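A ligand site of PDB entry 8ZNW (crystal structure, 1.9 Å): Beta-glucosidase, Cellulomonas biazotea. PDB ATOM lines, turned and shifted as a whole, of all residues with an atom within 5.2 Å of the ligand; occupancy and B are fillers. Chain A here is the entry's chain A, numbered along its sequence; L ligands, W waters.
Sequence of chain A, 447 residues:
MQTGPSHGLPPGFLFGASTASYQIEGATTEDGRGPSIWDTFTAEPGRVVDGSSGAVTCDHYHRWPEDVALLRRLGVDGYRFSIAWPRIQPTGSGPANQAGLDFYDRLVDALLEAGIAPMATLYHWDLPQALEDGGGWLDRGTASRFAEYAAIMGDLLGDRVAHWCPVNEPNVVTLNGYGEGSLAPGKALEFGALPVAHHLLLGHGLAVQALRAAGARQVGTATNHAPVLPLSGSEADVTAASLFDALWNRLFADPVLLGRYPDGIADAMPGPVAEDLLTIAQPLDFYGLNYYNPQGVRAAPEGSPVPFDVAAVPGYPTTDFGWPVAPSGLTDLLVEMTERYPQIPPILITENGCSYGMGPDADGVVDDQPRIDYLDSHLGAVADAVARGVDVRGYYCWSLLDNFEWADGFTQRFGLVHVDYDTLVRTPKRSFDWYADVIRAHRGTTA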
ATOM      1  N   ALA A  20      20.540  -8.232   8.351  1.00  0.00           N
ATOM      2  CA  ALA A  20      19.446  -8.912   7.686  1.00  0.00           C
ATOM      3  C   ALA A  20      18.431  -7.885   7.199  1.00  0.00           C
ATOM      4  O   ALA A  20      18.248  -6.790   7.765  1.00  0.00           O
ATOM      5  CB  ALA A  20      18.763  -9.954   8.547  1.00  0.00           C
ATOM      6  N   GLN A  23      15.471  -6.517   9.185  1.00  0.00           N
ATOM      7  CA  GLN A  23      15.942  -5.879  10.407  1.00  0.00           C
ATOM      8  C   GLN A  23      16.533  -4.489  10.142  1.00  0.00           C
ATOM      9  O   GLN A  23      16.456  -3.695  11.067  1.00  0.00           O
ATOM     10  CB  GLN A  23      16.958  -6.750  11.130  1.00  0.00           C
ATOM     11  CG  GLN A  23      16.388  -8.127  11.471  1.00  0.00           C
ATOM     12  CD  GLN A  23      17.344  -8.937  12.315  1.00  0.00           C
ATOM     13  OE1 GLN A  23      18.049  -9.805  11.819  1.00  0.00           O
ATOM     14  NE2 GLN A  23      17.372  -8.647  13.603  1.00  0.00           N
ATOM     15  N   HIS A 124      16.601 -14.915   5.181  1.00  0.00           N
ATOM     16  CA  HIS A 124      16.699 -14.538   6.571  1.00  0.00           C
ATOM     17  C   HIS A 124      15.311 -14.197   7.124  1.00  0.00           C
ATOM     18  O   HIS A 124      15.129 -13.132   7.727  1.00  0.00           O
ATOM     19  CB  HIS A 124      17.717 -13.397   6.715  1.00  0.00           C
ATOM     20  CG  HIS A 124      18.366 -13.294   8.054  1.00  0.00           C
ATOM     21  ND1 HIS A 124      19.738 -13.389   8.219  1.00  0.00           N
ATOM     22  CD2 HIS A 124      17.858 -13.170   9.297  1.00  0.00           C
ATOM     23  CE1 HIS A 124      20.017 -13.249   9.527  1.00  0.00           C
ATOM     24  NE2 HIS A 124      18.889 -13.111  10.202  1.00  0.00           N
ATOM     25  N   TRP A 125      14.371 -15.128   6.944  1.00  0.00           N
ATOM     26  CA  TRP A 125      13.124 -15.255   7.707  1.00  0.00           C
ATOM     27  C   TRP A 125      11.948 -14.458   7.126  1.00  0.00           C
ATOM     28  O   TRP A 125      10.832 -14.650   7.612  1.00  0.00           O
ATOM     29  CB  TRP A 125      13.307 -14.883   9.180  1.00  0.00           C
ATOM     30  CG  TRP A 125      14.394 -15.640   9.906  1.00  0.00           C
ATOM     31  CD1 TRP A 125      15.194 -16.641   9.449  1.00  0.00           C
ATOM     32  CD2 TRP A 125      14.760 -15.430  11.283  1.00  0.00           C
ATOM     33  NE1 TRP A 125      16.051 -17.051  10.430  1.00  0.00           N
ATOM     34  CE2 TRP A 125      15.795 -16.333  11.565  1.00  0.00           C
ATOM     35  CE3 TRP A 125      14.315 -14.568  12.277  1.00  0.00           C
ATOM     36  CZ2 TRP A 125      16.398 -16.393  12.828  1.00  0.00           C
ATOM     37  CZ3 TRP A 125      14.915 -14.620  13.508  1.00  0.00           C
ATOM     38  CH2 TRP A 125      15.916 -15.548  13.793  1.00  0.00           C
ATOM     39  N   ASN A 168      19.305 -18.811   6.676  1.00  0.00           N
ATOM     40  CA  ASN A 168      19.726 -18.453   8.012  1.00  0.00           C
ATOM     41  C   ASN A 168      18.941 -19.220   9.064  1.00  0.00           C
ATOM     42  O   ASN A 168      17.739 -19.095   9.173  1.00  0.00           O
ATOM     43  CB  ASN A 168      19.601 -16.940   8.238  1.00  0.00           C
ATOM     44  CG  ASN A 168      20.191 -16.528   9.571  1.00  0.00           C
ATOM     45  OD1 ASN A 168      21.399 -16.556   9.749  1.00  0.00           O
ATOM     46  ND2 ASN A 168      19.341 -16.189  10.524  1.00  0.00           N
ATOM     47  N   GLU A 169      19.665 -19.981   9.900  1.00  0.00           N
ATOM     48  CA  GLU A 169      19.154 -20.568  11.130  1.00  0.00           C
ATOM     49  C   GLU A 169      17.874 -21.345  10.869  1.00  0.00           C
ATOM     50  O   GLU A 169      16.785 -21.001  11.350  1.00  0.00           O
ATOM     51  CB  GLU A 169      18.981 -19.539  12.251  1.00  0.00           C
ATOM     52  CG  GLU A 169      20.286 -18.852  12.626  1.00  0.00           C
ATOM     53  CD  GLU A 169      20.229 -18.160  13.994  1.00  0.00           C
ATOM     54  OE1 GLU A 169      19.165 -17.967  14.484  1.00  0.00           O
ATOM     55  OE2 GLU A 169      21.259 -17.909  14.572  1.00  0.00           O
ATOM     56  N   ASN A 224      22.403 -21.955  13.294  1.00  0.00           N
ATOM     57  CA  ASN A 224      22.662 -21.644  14.694  1.00  0.00           C
ATOM     58  C   ASN A 224      23.175 -22.916  15.350  1.00  0.00           C
ATOM     59  O   ASN A 224      22.569 -23.957  15.149  1.00  0.00           O
ATOM     60  CB  ASN A 224      21.413 -21.122  15.388  1.00  0.00           C
ATOM     61  CG  ASN A 224      21.635 -20.779  16.845  1.00  0.00           C
ATOM     62  OD1 ASN A 224      21.785 -21.653  17.679  1.00  0.00           O
ATOM     63  ND2 ASN A 224      21.666 -19.501  17.152  1.00  0.00           N
ATOM     64  N   ASN A 290      26.301 -19.680  13.367  1.00  0.00           N
ATOM     65  CA  ASN A 290      25.961 -18.551  14.233  1.00  0.00           C
ATOM     66  C   ASN A 290      26.027 -19.052  15.678  1.00  0.00           C
ATOM     67  O   ASN A 290      25.404 -20.062  16.023  1.00  0.00           O
ATOM     68  CB  ASN A 290      24.563 -17.999  13.985  1.00  0.00           C
ATOM     69  CG  ASN A 290      24.322 -17.554  12.556  1.00  0.00           C
ATOM     70  OD1 ASN A 290      25.269 -17.359  11.800  1.00  0.00           O
ATOM     71  ND2 ASN A 290      23.068 -17.241  12.247  1.00  0.00           N
ATOM     72  N   TYR A 292      26.003 -17.755  19.813  1.00  0.00           N
ATOM     73  CA  TYR A 292      25.839 -16.710  20.813  1.00  0.00           C
ATOM     74  C   TYR A 292      26.236 -17.215  22.211  1.00  0.00           C
ATOM     75  O   TYR A 292      26.873 -16.480  22.971  1.00  0.00           O
ATOM     76  CB  TYR A 292      24.410 -16.132  20.801  1.00  0.00           C
ATOM     77  CG  TYR A 292      24.166 -15.333  19.543  1.00  0.00           C
ATOM     78  CD1 TYR A 292      24.482 -13.979  19.517  1.00  0.00           C
ATOM     79  CD2 TYR A 292      23.799 -15.951  18.352  1.00  0.00           C
ATOM     80  CE1 TYR A 292      24.325 -13.226  18.369  1.00  0.00           C
ATOM     81  CE2 TYR A 292      23.732 -15.229  17.174  1.00  0.00           C
ATOM     82  CZ  TYR A 292      23.961 -13.862  17.201  1.00  0.00           C
ATOM     83  OH  TYR A 292      23.841 -13.057  16.118  1.00  0.00           O
ATOM     84  N   PHE A 321      20.287  -8.817  27.075  1.00  0.00           N
ATOM     85  CA  PHE A 321      19.218  -9.704  26.691  1.00  0.00           C
ATOM     86  C   PHE A 321      19.034 -10.834  27.714  1.00  0.00           C
ATOM     87  O   PHE A 321      18.196 -11.718  27.487  1.00  0.00           O
ATOM     88  CB  PHE A 321      19.503 -10.299  25.307  1.00  0.00           C
ATOM     89  CG  PHE A 321      18.362 -10.439  24.320  1.00  0.00           C
ATOM     90  CD1 PHE A 321      17.052 -10.636  24.724  1.00  0.00           C
ATOM     91  CD2 PHE A 321      18.621 -10.355  22.962  1.00  0.00           C
ATOM     92  CE1 PHE A 321      16.037 -10.798  23.790  1.00  0.00           C
ATOM     93  CE2 PHE A 321      17.608 -10.495  22.024  1.00  0.00           C
ATOM     94  CZ  PHE A 321      16.309 -10.709  22.439  1.00  0.00           C
ATOM     95  N   TRP A 323      21.334 -13.104  28.231  1.00  0.00           N
ATOM     96  CA  TRP A 323      22.054 -14.248  27.683  1.00  0.00           C
ATOM     97  C   TRP A 323      23.402 -14.415  28.362  1.00  0.00           C
ATOM     98  O   TRP A 323      24.111 -13.431  28.576  1.00  0.00           O
ATOM     99  CB  TRP A 323      22.264 -14.108  26.172  1.00  0.00           C
ATOM    100  CG  TRP A 323      20.984 -14.062  25.370  1.00  0.00           C
ATOM    101  CD1 TRP A 323      19.714 -14.187  25.834  1.00  0.00           C
ATOM    102  CD2 TRP A 323      20.885 -13.852  23.942  1.00  0.00           C
ATOM    103  NE1 TRP A 323      18.835 -14.090  24.787  1.00  0.00           N
ATOM    104  CE2 TRP A 323      19.504 -13.878  23.621  1.00  0.00           C
ATOM    105  CE3 TRP A 323      21.816 -13.649  22.915  1.00  0.00           C
ATOM    106  CZ2 TRP A 323      19.036 -13.705  22.321  1.00  0.00           C
ATOM    107  CZ3 TRP A 323      21.337 -13.457  21.636  1.00  0.00           C
ATOM    108  CH2 TRP A 323      19.977 -13.484  21.342  1.00  0.00           C
ATOM    109  N   GLU A 351      27.795 -15.343  12.357  1.00  0.00           N
ATOM    110  CA  GLU A 351      27.278 -14.392  13.333  1.00  0.00           C
ATOM    111  C   GLU A 351      27.837 -14.728  14.731  1.00  0.00           C
ATOM    112  O   GLU A 351      27.869 -15.877  15.182  1.00  0.00           O
ATOM    113  CB  GLU A 351      25.747 -14.410  13.505  1.00  0.00           C
ATOM    114  CG  GLU A 351      24.945 -14.038  12.284  1.00  0.00           C
ATOM    115  CD  GLU A 351      23.436 -14.001  12.513  1.00  0.00           C
ATOM    116  OE1 GLU A 351      22.697 -14.074  11.498  1.00  0.00           O
ATOM    117  OE2 GLU A 351      23.013 -13.804  13.720  1.00  0.00           O
ATOM    118  N   TRP A 398      27.696  -9.810  14.458  1.00  0.00           N
ATOM    119  CA  TRP A 398      26.306  -9.344  14.476  1.00  0.00           C
ATOM    120  C   TRP A 398      26.230  -8.201  15.477  1.00  0.00           C
ATOM    121  O   TRP A 398      26.408  -8.438  16.678  1.00  0.00           O
ATOM    122  CB  TRP A 398      25.307 -10.453  14.857  1.00  0.00           C
ATOM    123  CG  TRP A 398      23.909  -9.938  14.700  1.00  0.00           C
ATOM    124  CD1 TRP A 398      23.161  -9.283  15.634  1.00  0.00           C
ATOM    125  CD2 TRP A 398      23.145  -9.904  13.496  1.00  0.00           C
ATOM    126  NE1 TRP A 398      21.970  -8.864  15.100  1.00  0.00           N
ATOM    127  CE2 TRP A 398      21.930  -9.235  13.787  1.00  0.00           C
ATOM    128  CE3 TRP A 398      23.350 -10.385  12.198  1.00  0.00           C
ATOM    129  CZ2 TRP A 398      20.957  -9.019  12.819  1.00  0.00           C
ATOM    130  CZ3 TRP A 398      22.383 -10.196  11.253  1.00  0.00           C
ATOM    131  CH2 TRP A 398      21.204  -9.523  11.555  1.00  0.00           C
ATOM    132  N   ASN A 403      19.482  -2.609  15.221  1.00  0.00           N
ATOM    133  CA  ASN A 403      18.421  -2.897  14.279  1.00  0.00           C
ATOM    134  C   ASN A 403      17.186  -3.465  14.969  1.00  0.00           C
ATOM    135  O   ASN A 403      17.120  -3.538  16.187  1.00  0.00           O
ATOM    136  CB  ASN A 403      18.974  -3.768  13.163  1.00  0.00           C
ATOM    137  CG  ASN A 403      19.454  -5.096  13.660  1.00  0.00           C
ATOM    138  OD1 ASN A 403      18.679  -5.861  14.215  1.00  0.00           O
ATOM    139  ND2 ASN A 403      20.707  -5.417  13.392  1.00  0.00           N
ATOM    140  N   GLU A 405      15.143  -6.163  16.373  1.00  0.00           N
ATOM    141  CA  GLU A 405      15.411  -7.496  16.897  1.00  0.00           C
ATOM    142  C   GLU A 405      14.092  -8.250  17.042  1.00  0.00           C
ATOM    143  O   GLU A 405      13.667  -8.564  18.158  1.00  0.00           O
ATOM    144  CB  GLU A 405      16.108  -7.310  18.239  1.00  0.00           C
ATOM    145  CG  GLU A 405      16.597  -8.579  18.923  1.00  0.00           C
ATOM    146  CD  GLU A 405      17.374  -9.541  18.045  1.00  0.00           C
ATOM    147  OE1 GLU A 405      17.231 -10.753  18.240  1.00  0.00           O
ATOM    148  OE2 GLU A 405      18.132  -9.064  17.134  1.00  0.00           O
ATOM    149  N   TRP A 406      13.415  -8.478  15.911  1.00  0.00           N
ATOM    150  CA  TRP A 406      12.334  -9.425  15.824  1.00  0.00           C
ATOM    151  C   TRP A 406      11.296  -9.097  16.904  1.00  0.00           C
ATOM    152  O   TRP A 406      10.899  -7.930  17.043  1.00  0.00           O
ATOM    153  CB  TRP A 406      12.933 -10.844  15.883  1.00  0.00           C
ATOM    154  CG  TRP A 406      13.976 -11.063  14.804  1.00  0.00           C
ATOM    155  CD1 TRP A 406      15.281 -11.430  14.971  1.00  0.00           C
ATOM    156  CD2 TRP A 406      13.763 -10.971  13.375  1.00  0.00           C
ATOM    157  NE1 TRP A 406      15.916 -11.568  13.759  1.00  0.00           N
ATOM    158  CE2 TRP A 406      15.001 -11.300  12.755  1.00  0.00           C
ATOM    159  CE3 TRP A 406      12.667 -10.653  12.549  1.00  0.00           C
ATOM    160  CZ2 TRP A 406      15.155 -11.311  11.380  1.00  0.00           C
ATOM    161  CZ3 TRP A 406      12.821 -10.707  11.191  1.00  0.00           C
ATOM    162  CH2 TRP A 406      14.053 -11.024  10.603  1.00  0.00           C
ATOM    163  N   PHE A 414      22.439  -4.539  19.146  1.00  0.00           N
ATOM    164  CA  PHE A 414      23.558  -5.408  18.820  1.00  0.00           C
ATOM    165  C   PHE A 414      24.667  -4.725  18.009  1.00  0.00           C
ATOM    166  O   PHE A 414      25.690  -5.349  17.731  1.00  0.00           O
ATOM    167  CB  PHE A 414      23.099  -6.624  18.041  1.00  0.00           C
ATOM    168  CG  PHE A 414      22.499  -7.755  18.853  1.00  0.00           C
ATOM    169  CD1 PHE A 414      21.181  -7.720  19.251  1.00  0.00           C
ATOM    170  CD2 PHE A 414      23.286  -8.831  19.274  1.00  0.00           C
ATOM    171  CE1 PHE A 414      20.631  -8.740  19.998  1.00  0.00           C
ATOM    172  CE2 PHE A 414      22.748  -9.866  20.042  1.00  0.00           C
ATOM    173  CZ  PHE A 414      21.403  -9.836  20.353  1.00  0.00           C
HETATM  174  C1  LIG L   1      19.715 -13.909  13.918  1.00  0.00           C
HETATM  175  C2  LIG L   1      19.624 -12.401  13.873  1.00  0.00           C
HETATM  176  C3  LIG L   1      19.282 -11.860  15.261  1.00  0.00           C
HETATM  177  C4  LIG L   1      20.344 -12.308  16.276  1.00  0.00           C
HETATM  178  C5  LIG L   1      20.084 -11.893  17.706  1.00  0.00           C
HETATM  179  C6  LIG L   1      20.480 -14.374  15.092  1.00  0.00           C
HETATM  180  O1  LIG L   1      20.406 -15.688  15.286  1.00  0.00           O
HETATM  181  O2  LIG L   1      20.207 -14.497  12.728  1.00  0.00           O
HETATM  182  O3  LIG L   1      18.631 -12.074  12.901  1.00  0.00           O
HETATM  183  O4  LIG L   1      19.221 -10.444  15.276  1.00  0.00           O
HETATM  184  O5  LIG L   1      20.355 -13.705  16.335  1.00  0.00           O
HETATM  185  O6  LIG L   1      18.996 -12.643  18.207  1.00  0.00           O
HETATM  186  O   HOH W   1      19.704  -7.241  16.273  1.00  0.00           O
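Asn 290 touches the ligand. OH of Tyr 292 touches O5 of the ligand (3.6 Å). Trp 323 touches the ligand (CH2 to O6, 3.4 Å). CZ of Phe 414 touches C5 of the ligand (3.6 Å). Hydrophobic or aromatic side chains that line the ligand: His 124, Tyr 292, Trp 323, Trp 398, Trp 406 and Phe 414. The nearest printed residue that does not touch the ligand is Trp 125 (4.1 Å).
The side-chain carboxylate of Glu 169 is in hydrogen-bond range of an oxygen (O1) of the ligand (2.5 Å). OE2 of Glu 405 lies within hydrogen-bond range of O4 of the ligand, at 2.6 Å. The side-chain amide oxygen of Gln 23 is in hydrogen-bond range of an oxygen (O3) of the ligand. The side-chain carboxylate (OE1) of Glu 351 is in hydrogen-bond range of an oxygen (O2) of the ligand (2.8 Å). O3 of the ligand sits at hydrogen-bond distance from NE1 of Trp 406. An oxygen (O3) of the ligand sits at hydrogen-bond distance from a ring nitrogen (NE2) of His 124, at 2.9 Å. O2 of the ligand sits at hydrogen-bond distance from ND2 of Asn 168, at 2.9 Å. An oxygen (O4) of the ligand lies within hydrogen-bond range of the indole nitrogen of Trp 398, 3.2 Å away.
Water W1 lies within hydrogen-bond range of OE2 of Glu 405 (2.6 Å), OD1 of Asn 403 (2.7 Å), NE1 of Trp 398 (3.0 Å) and O4 of the ligand (3.4 Å).
The side-chain carboxylate of Glu 169 is in hydrogen-bond range of the side-chain amide nitrogen of Asn 290, 3.0 Å away. The indole nitrogen of Trp 406 lies close to the side-chain amide nitrogen of Gln 23, 3.3 Å away. The side-chain amide nitrogen of Gln 23 lies within hydrogen-bond range of the side-chain amide oxygen of Asn 403 (3.1 Å). OE1 of Glu 351 lies close to OD1 of Asn 168 (3.3 Å). The side-chain carboxylate of Glu 351 is in hydrogen-bond range of the side-chain hydroxyl of Tyr 292. OE1 of Glu 351 lies close to ND2 of Asn 290. A ring nitrogen (NE2) of His 124 sits at hydrogen-bond distance from the side-chain amide nitrogen (ND2) of Asn 168. The side-chain amide oxygen of Asn 168 sits at hydrogen-bond distance from the side-chain amide nitrogen of Asn 290 (3.1 Å).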
